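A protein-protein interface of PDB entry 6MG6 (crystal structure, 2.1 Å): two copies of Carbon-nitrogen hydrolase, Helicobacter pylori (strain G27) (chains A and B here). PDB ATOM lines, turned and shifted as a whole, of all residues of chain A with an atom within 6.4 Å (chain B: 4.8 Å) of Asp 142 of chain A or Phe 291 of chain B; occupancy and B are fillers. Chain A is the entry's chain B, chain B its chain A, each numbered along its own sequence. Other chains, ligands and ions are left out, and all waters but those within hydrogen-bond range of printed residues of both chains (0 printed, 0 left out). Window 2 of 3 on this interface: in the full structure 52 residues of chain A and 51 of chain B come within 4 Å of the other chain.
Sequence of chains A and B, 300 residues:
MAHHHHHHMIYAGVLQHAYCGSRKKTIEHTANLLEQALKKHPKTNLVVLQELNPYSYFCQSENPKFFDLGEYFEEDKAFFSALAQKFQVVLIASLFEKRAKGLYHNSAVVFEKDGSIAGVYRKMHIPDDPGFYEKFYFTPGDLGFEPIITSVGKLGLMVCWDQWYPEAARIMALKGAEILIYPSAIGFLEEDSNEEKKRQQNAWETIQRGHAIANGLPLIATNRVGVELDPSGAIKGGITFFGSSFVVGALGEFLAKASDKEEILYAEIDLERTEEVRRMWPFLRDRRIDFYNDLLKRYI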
ATOM      1  N   ARG A  99     -25.153  21.551  -0.815  1.00  0.00           N
ATOM      2  CA  ARG A  99     -23.872  21.158  -1.390  1.00  0.00           C
ATOM      3  C   ARG A  99     -22.715  21.506  -0.466  1.00  0.00           C
ATOM      4  O   ARG A  99     -21.734  20.765  -0.386  1.00  0.00           O
ATOM      5  CB  ARG A  99     -23.699  21.852  -2.740  1.00  0.00           C
ATOM      6  CG  ARG A  99     -22.372  21.579  -3.426  1.00  0.00           C
ATOM      7  CD  ARG A  99     -22.576  20.491  -4.448  1.00  0.00           C
ATOM      8  NE  ARG A  99     -21.380  20.201  -5.224  1.00  0.00           N
ATOM      9  CZ  ARG A  99     -21.173  20.621  -6.469  1.00  0.00           C
ATOM     10  NH1 ARG A  99     -22.071  21.370  -7.078  1.00  0.00           N
ATOM     11  NH2 ARG A  99     -20.058  20.285  -7.109  1.00  0.00           N
ATOM     12  N   HIS A 105     -28.658  23.268  -4.009  1.00  0.00           N
ATOM     13  CA  HIS A 105     -29.235  22.926  -5.308  1.00  0.00           C
ATOM     14  C   HIS A 105     -30.668  22.418  -5.157  1.00  0.00           C
ATOM     15  O   HIS A 105     -31.061  21.897  -4.111  1.00  0.00           O
ATOM     16  CB  HIS A 105     -28.428  21.846  -6.018  1.00  0.00           C
ATOM     17  CG  HIS A 105     -27.022  22.242  -6.322  1.00  0.00           C
ATOM     18  ND1 HIS A 105     -26.699  23.158  -7.301  1.00  0.00           N
ATOM     19  CD2 HIS A 105     -25.848  21.841  -5.779  1.00  0.00           C
ATOM     20  CE1 HIS A 105     -25.387  23.295  -7.355  1.00  0.00           C
ATOM     21  NE2 HIS A 105     -24.847  22.506  -6.442  1.00  0.00           N
ATOM     22  N   ARG A 122     -29.294  17.798 -10.686  1.00  0.00           N
ATOM     23  CA  ARG A 122     -29.419  19.146 -10.145  1.00  0.00           C
ATOM     24  C   ARG A 122     -30.107  20.031 -11.173  1.00  0.00           C
ATOM     25  O   ARG A 122     -29.628  20.149 -12.306  1.00  0.00           O
ATOM     26  CB  ARG A 122     -28.047  19.706  -9.777  1.00  0.00           C
ATOM     27  CG  ARG A 122     -27.419  18.978  -8.616  1.00  0.00           C
ATOM     28  CD  ARG A 122     -25.981  19.392  -8.406  1.00  0.00           C
ATOM     29  NE  ARG A 122     -25.425  18.700  -7.250  1.00  0.00           N
ATOM     30  CZ  ARG A 122     -24.139  18.408  -7.090  1.00  0.00           C
ATOM     31  NH1 ARG A 122     -23.248  18.744  -8.024  1.00  0.00           N
ATOM     32  NH2 ARG A 122     -23.749  17.764  -6.002  1.00  0.00           N
ATOM     33  N   LYS A 123     -31.237  20.633 -10.789  1.00  0.00           N
ATOM     34  CA  LYS A 123     -31.951  21.537 -11.683  1.00  0.00           C
ATOM     35  C   LYS A 123     -30.991  22.492 -12.393  1.00  0.00           C
ATOM     36  O   LYS A 123     -30.139  23.117 -11.761  1.00  0.00           O
ATOM     37  CB  LYS A 123     -32.984  22.328 -10.890  1.00  0.00           C
ATOM     38  CG  LYS A 123     -33.983  23.087 -11.755  1.00  0.00           C
ATOM     39  CD  LYS A 123     -35.047  23.711 -10.836  1.00  0.00           C
ATOM     40  CE  LYS A 123     -36.167  24.370 -11.632  1.00  0.00           C
ATOM     41  NZ  LYS A 123     -37.332  24.604 -10.720  1.00  0.00           N
ATOM     42  N   MET A 124     -31.113  22.570 -13.717  1.00  0.00           N
ATOM     43  CA  MET A 124     -30.173  23.329 -14.535  1.00  0.00           C
ATOM     44  C   MET A 124     -30.665  24.743 -14.826  1.00  0.00           C
ATOM     45  O   MET A 124     -29.922  25.706 -14.657  1.00  0.00           O
ATOM     46  CB  MET A 124     -29.877  22.572 -15.839  1.00  0.00           C
ATOM     47  CG  MET A 124     -28.987  21.326 -15.639  1.00  0.00           C
ATOM     48  SD  MET A 124     -27.289  21.677 -15.137  1.00  0.00           S
ATOM     49  CE  MET A 124     -26.637  22.429 -16.640  1.00  0.00           C
ATOM     50  N   THR A 139     -28.346  27.222  -6.589  1.00  0.00           N
ATOM     51  CA  THR A 139     -27.242  27.331  -7.503  1.00  0.00           C
ATOM     52  C   THR A 139     -27.557  26.498  -8.734  1.00  0.00           C
ATOM     53  O   THR A 139     -27.974  25.341  -8.591  1.00  0.00           O
ATOM     54  CB  THR A 139     -25.968  26.860  -6.807  1.00  0.00           C
ATOM     55  OG1 THR A 139     -25.738  27.716  -5.675  1.00  0.00           O
ATOM     56  CG2 THR A 139     -24.778  26.951  -7.745  1.00  0.00           C
ATOM     57  N   PRO A 140     -27.392  27.042  -9.945  1.00  0.00           N
ATOM     58  CA  PRO A 140     -27.698  26.259 -11.153  1.00  0.00           C
ATOM     59  C   PRO A 140     -26.863  24.990 -11.170  1.00  0.00           C
ATOM     60  O   PRO A 140     -25.723  24.981 -10.718  1.00  0.00           O
ATOM     61  CB  PRO A 140     -27.312  27.204 -12.304  1.00  0.00           C
ATOM     62  CG  PRO A 140     -27.379  28.603 -11.684  1.00  0.00           C
ATOM     63  CD  PRO A 140     -26.942  28.411 -10.251  1.00  0.00           C
ATOM     64  N   GLY A 141     -27.466  23.902 -11.646  1.00  0.00           N
ATOM     65  CA  GLY A 141     -26.776  22.626 -11.649  1.00  0.00           C
ATOM     66  C   GLY A 141     -25.491  22.694 -12.445  1.00  0.00           C
ATOM     67  O   GLY A 141     -25.360  23.462 -13.407  1.00  0.00           O
ATOM     68  N   ASP A 142     -24.527  21.871 -12.040  1.00  0.00           N
ATOM     69  CA  ASP A 142     -23.231  21.870 -12.694  1.00  0.00           C
ATOM     70  C   ASP A 142     -22.850  20.528 -13.294  1.00  0.00           C
ATOM     71  O   ASP A 142     -21.763  20.415 -13.859  1.00  0.00           O
ATOM     72  CB  ASP A 142     -22.142  22.326 -11.713  1.00  0.00           C
ATOM     73  CG  ASP A 142     -22.055  21.444 -10.457  1.00  0.00           C
ATOM     74  OD1 ASP A 142     -23.050  20.759 -10.093  1.00  0.00           O
ATOM     75  OD2 ASP A 142     -20.972  21.441  -9.838  1.00  0.00           O
ATOM     76  N   LEU A 143     -23.701  19.518 -13.185  1.00  0.00           N
ATOM     77  CA  LEU A 143     -23.438  18.219 -13.790  1.00  0.00           C
ATOM     78  C   LEU A 143     -23.920  18.139 -15.233  1.00  0.00           C
ATOM     79  O   LEU A 143     -23.491  17.244 -15.968  1.00  0.00           O
ATOM     80  CB  LEU A 143     -24.127  17.113 -12.989  1.00  0.00           C
ATOM     81  CG  LEU A 143     -23.904  17.041 -11.482  1.00  0.00           C
ATOM     82  CD1 LEU A 143     -25.156  16.445 -10.786  1.00  0.00           C
ATOM     83  CD2 LEU A 143     -22.675  16.217 -11.191  1.00  0.00           C
ATOM     84  N   GLY A 144     -24.794  19.045 -15.651  1.00  0.00           N
ATOM     85  CA  GLY A 144     -25.302  19.024 -16.998  1.00  0.00           C
ATOM     86  C   GLY A 144     -26.504  18.115 -17.113  1.00  0.00           C
ATOM     87  O   GLY A 144     -27.170  17.767 -16.134  1.00  0.00           O
ATOM     88  N   PHE A 145     -26.804  17.759 -18.351  1.00  0.00           N
ATOM     89  CA  PHE A 145     -28.002  16.991 -18.679  1.00  0.00           C
ATOM     90  C   PHE A 145     -27.566  15.553 -18.911  1.00  0.00           C
ATOM     91  O   PHE A 145     -27.172  15.189 -20.013  1.00  0.00           O
ATOM     92  CB  PHE A 145     -28.696  17.591 -19.889  1.00  0.00           C
ATOM     93  CG  PHE A 145     -28.984  19.059 -19.733  1.00  0.00           C
ATOM     94  CD1 PHE A 145     -28.188  20.007 -20.340  1.00  0.00           C
ATOM     95  CD2 PHE A 145     -30.053  19.481 -18.946  1.00  0.00           C
ATOM     96  CE1 PHE A 145     -28.452  21.358 -20.180  1.00  0.00           C
ATOM     97  CE2 PHE A 145     -30.326  20.833 -18.786  1.00  0.00           C
ATOM     98  CZ  PHE A 145     -29.529  21.768 -19.402  1.00  0.00           C
ATOM     99  N   ILE A 171     -30.750  16.861 -25.399  1.00  0.00           N
ATOM    100  CA  ILE A 171     -29.486  16.336 -24.890  1.00  0.00           C
ATOM    101  C   ILE A 171     -29.704  15.028 -24.130  1.00  0.00           C
ATOM    102  O   ILE A 171     -28.930  14.075 -24.287  1.00  0.00           O
ATOM    103  CB  ILE A 171     -28.769  17.390 -24.020  1.00  0.00           C
ATOM    104  CG1 ILE A 171     -28.243  18.526 -24.900  1.00  0.00           C
ATOM    105  CG2 ILE A 171     -27.612  16.763 -23.226  1.00  0.00           C
ATOM    106  CD1 ILE A 171     -27.871  19.782 -24.123  1.00  0.00           C
ATOM    107  N   LEU A 296     -25.253  27.817 -29.026  1.00  0.00           N
ATOM    108  CA  LEU A 296     -24.370  28.104 -27.899  1.00  0.00           C
ATOM    109  C   LEU A 296     -24.314  29.584 -27.564  1.00  0.00           C
ATOM    110  O   LEU A 296     -23.623  29.964 -26.618  1.00  0.00           O
ATOM    111  CB  LEU A 296     -22.957  27.600 -28.197  1.00  0.00           C
ATOM    112  CG  LEU A 296     -22.845  26.122 -28.570  1.00  0.00           C
ATOM    113  CD1 LEU A 296     -21.392  25.742 -28.720  1.00  0.00           C
ATOM    114  CD2 LEU A 296     -23.544  25.250 -27.541  1.00  0.00           C
ATOM    115  N   ARG B 288     -29.274  27.576 -20.518  1.00  0.00           N
ATOM    116  CA  ARG B 288     -27.963  27.170 -19.993  1.00  0.00           C
ATOM    117  C   ARG B 288     -27.001  26.875 -21.149  1.00  0.00           C
ATOM    118  O   ARG B 288     -26.530  25.754 -21.347  1.00  0.00           O
ATOM    119  CB  ARG B 288     -28.104  25.963 -19.063  1.00  0.00           C
ATOM    120  CG  ARG B 288     -28.771  26.263 -17.686  1.00  0.00           C
ATOM    121  CD  ARG B 288     -27.934  27.259 -16.825  1.00  0.00           C
ATOM    122  NE  ARG B 288     -26.540  26.815 -16.631  1.00  0.00           N
ATOM    123  CZ  ARG B 288     -26.138  25.912 -15.724  1.00  0.00           C
ATOM    124  NH1 ARG B 288     -27.004  25.315 -14.904  1.00  0.00           N
ATOM    125  NH2 ARG B 288     -24.851  25.598 -15.624  1.00  0.00           N
ATOM    126  N   ILE B 289     -26.668  27.930 -21.894  1.00  0.00           N
ATOM    127  CA  ILE B 289     -25.827  27.756 -23.072  1.00  0.00           C
ATOM    128  C   ILE B 289     -24.457  27.194 -22.712  1.00  0.00           C
ATOM    129  O   ILE B 289     -23.780  26.625 -23.576  1.00  0.00           O
ATOM    130  CB  ILE B 289     -25.680  29.087 -23.845  1.00  0.00           C
ATOM    131  CG1 ILE B 289     -25.024  30.157 -22.980  1.00  0.00           C
ATOM    132  CG2 ILE B 289     -27.072  29.586 -24.295  1.00  0.00           C
ATOM    133  CD1 ILE B 289     -24.855  31.537 -23.717  1.00  0.00           C
ATOM    134  N   ASP B 290     -24.023  27.337 -21.457  1.00  0.00           N
ATOM    135  CA  ASP B 290     -22.757  26.732 -21.050  1.00  0.00           C
ATOM    136  C   ASP B 290     -22.823  25.201 -21.015  1.00  0.00           C
ATOM    137  O   ASP B 290     -21.774  24.558 -20.944  1.00  0.00           O
ATOM    138  CB  ASP B 290     -22.309  27.256 -19.672  1.00  0.00           C
ATOM    139  CG  ASP B 290     -23.391  27.087 -18.568  1.00  0.00           C
ATOM    140  OD1 ASP B 290     -24.605  27.125 -18.836  1.00  0.00           O
ATOM    141  OD2 ASP B 290     -23.012  26.898 -17.413  1.00  0.00           O
ATOM    142  N   PHE B 291     -24.013  24.602 -21.094  1.00  0.00           N
ATOM    143  CA  PHE B 291     -24.159  23.144 -21.128  1.00  0.00           C
ATOM    144  C   PHE B 291     -24.962  22.678 -22.342  1.00  0.00           C
ATOM    145  O   PHE B 291     -25.585  21.617 -22.302  1.00  0.00           O
ATOM    146  CB  PHE B 291     -24.789  22.614 -19.829  1.00  0.00           C
ATOM    147  CG  PHE B 291     -23.790  22.458 -18.701  1.00  0.00           C
ATOM    148  CD1 PHE B 291     -23.426  23.550 -17.918  1.00  0.00           C
ATOM    149  CD2 PHE B 291     -23.165  21.237 -18.479  1.00  0.00           C
ATOM    150  CE1 PHE B 291     -22.466  23.430 -16.899  1.00  0.00           C
ATOM    151  CE2 PHE B 291     -22.215  21.094 -17.474  1.00  0.00           C
ATOM    152  CZ  PHE B 291     -21.876  22.198 -16.667  1.00  0.00           C
ATOM    153  N   TYR B 292     -24.950  23.437 -23.441  1.00  0.00           N
ATOM    154  CA  TYR B 292     -25.672  23.037 -24.646  1.00  0.00           C
ATOM    155  C   TYR B 292     -24.772  22.418 -25.699  1.00  0.00           C
ATOM    156  O   TYR B 292     -25.264  22.024 -26.755  1.00  0.00           O
ATOM    157  CB  TYR B 292     -26.398  24.228 -25.273  1.00  0.00           C
ATOM    158  CG  TYR B 292     -27.657  24.649 -24.546  1.00  0.00           C
ATOM    159  CD1 TYR B 292     -28.147  23.919 -23.469  1.00  0.00           C
ATOM    160  CD2 TYR B 292     -28.343  25.796 -24.931  1.00  0.00           C
ATOM    161  CE1 TYR B 292     -29.324  24.331 -22.781  1.00  0.00           C
ATOM    162  CE2 TYR B 292     -29.477  26.210 -24.254  1.00  0.00           C
ATOM    163  CZ  TYR B 292     -29.967  25.482 -23.195  1.00  0.00           C
ATOM    164  OH  TYR B 292     -31.123  25.941 -22.584  1.00  0.00           O
ATOM    165  N   ASN B 293     -23.476  22.297 -25.418  1.00  0.00           N
ATOM    166  CA  ASN B 293     -22.508  21.820 -26.405  1.00  0.00           C
ATOM    167  C   ASN B 293     -22.889  20.456 -26.973  1.00  0.00           C
ATOM    168  O   ASN B 293     -22.590  20.168 -28.132  1.00  0.00           O
ATOM    169  CB  ASN B 293     -21.123  21.745 -25.753  1.00  0.00           C
ATOM    170  CG  ASN B 293     -20.644  23.101 -25.240  1.00  0.00           C
ATOM    171  OD1 ASN B 293     -21.161  23.615 -24.251  1.00  0.00           O
ATOM    172  ND2 ASN B 293     -19.605  23.635 -25.856  1.00  0.00           N
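NH1 of Arg 288 of chain B lies within hydrogen-bond range of O of Met 124 of chain A (3.0 Å).
The guanidinium group of Arg 288 of chain B sits at hydrogen-bond distance from the backbone carbonyl oxygen of Gly 141 of chain A (2.9 Å).
The side-chain carboxylate (OD2) of Asp 290 of chain B is in salt-bridge range of the guanidinium group (NH2) of Arg 288 of chain B, 2.9 Å away.
N of Arg 288 of chain B is in hydrogen-bond range of OH of Tyr 292 of chain B (3.2 Å).
OD1 of Asn 293 of chain B sits close to O of Asp 290 of chain B, 3.5 Å away.
The guanidinium group (NH1) of Arg 122 of chain A is in salt-bridge range of the side-chain carboxylate (OD1) of Asp 142 of chain A, at 2.9 Å.
The backbone carbonyl oxygen of Lys 123 of chain A lies within hydrogen-bond range of the backbone NH of Gly 141 of chain A.
SD of Met 124 of chain A lies within hydrogen-bond range of N of Gly 144 of chain A (3.7 Å).
Among the printed residues, pairs that only touch across the chains: Met 124 of chain A with Phe 291 of chain B (3.5 Å), Pro 140 of chain A with Arg 288 of chain B (3.2 Å), Asp 142 of chain A with Phe 291 of chain B (3.3 Å), Gly 144 of chain A with Phe 291 of chain B (3.4 Å), Phe 145 of chain A with Phe 291 of chain B (3.6 Å), Ile 171 of chain A with Phe 291 of chain B (3.5 Å), Ile 171 of chain A with Tyr 292 of chain B (3.96 Å), Leu 296 of chain A with Ile 289 of chain B (3.5 Å), Leu 296 of chain A with Tyr 292 of chain B (3.6 Å) and Leu 296 of chain A with Asn 293 of chain B (3.6 Å).
Of the printed residues of chain B, Gly 141 of chain A touches Arg 288.
Printed residues of chain B within 4 Å of Ile 171 of chain A: Phe 291 and Tyr 292.
Printed residues of chain B within 4 Å of Leu 296 of chain A: Ile 289 (3.5 Å), Tyr 292 (3.6 Å) and Asn 293 (3.6 Å).
Phe 291 of chain B touches just these residues of chain A: Met 124, Asp 142, Gly 144, Phe 145 and Ile 171.
Printed residues of chain A within 4 Å of Asn 293 of chain B: Leu 296 (3.6 Å).
The nearest printed residue of chain B that does not touch Asp 142 of chain A is Arg 288 of chain B (5.0 Å).
Hydrophobic or aromatic side chains of chain B within 4 Å of the printed part of chain A: Ile 289, Phe 291 and Tyr 292.
Of the 14 printed residues of chain A, 8 touch a printed residue of chain B.
Hydrophobic or aromatic side chains of chain A that line the printed part of chain B: Met 124, Pro 140, Phe 145, Ile 171 and Leu 296.
No position is printed for both chains.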
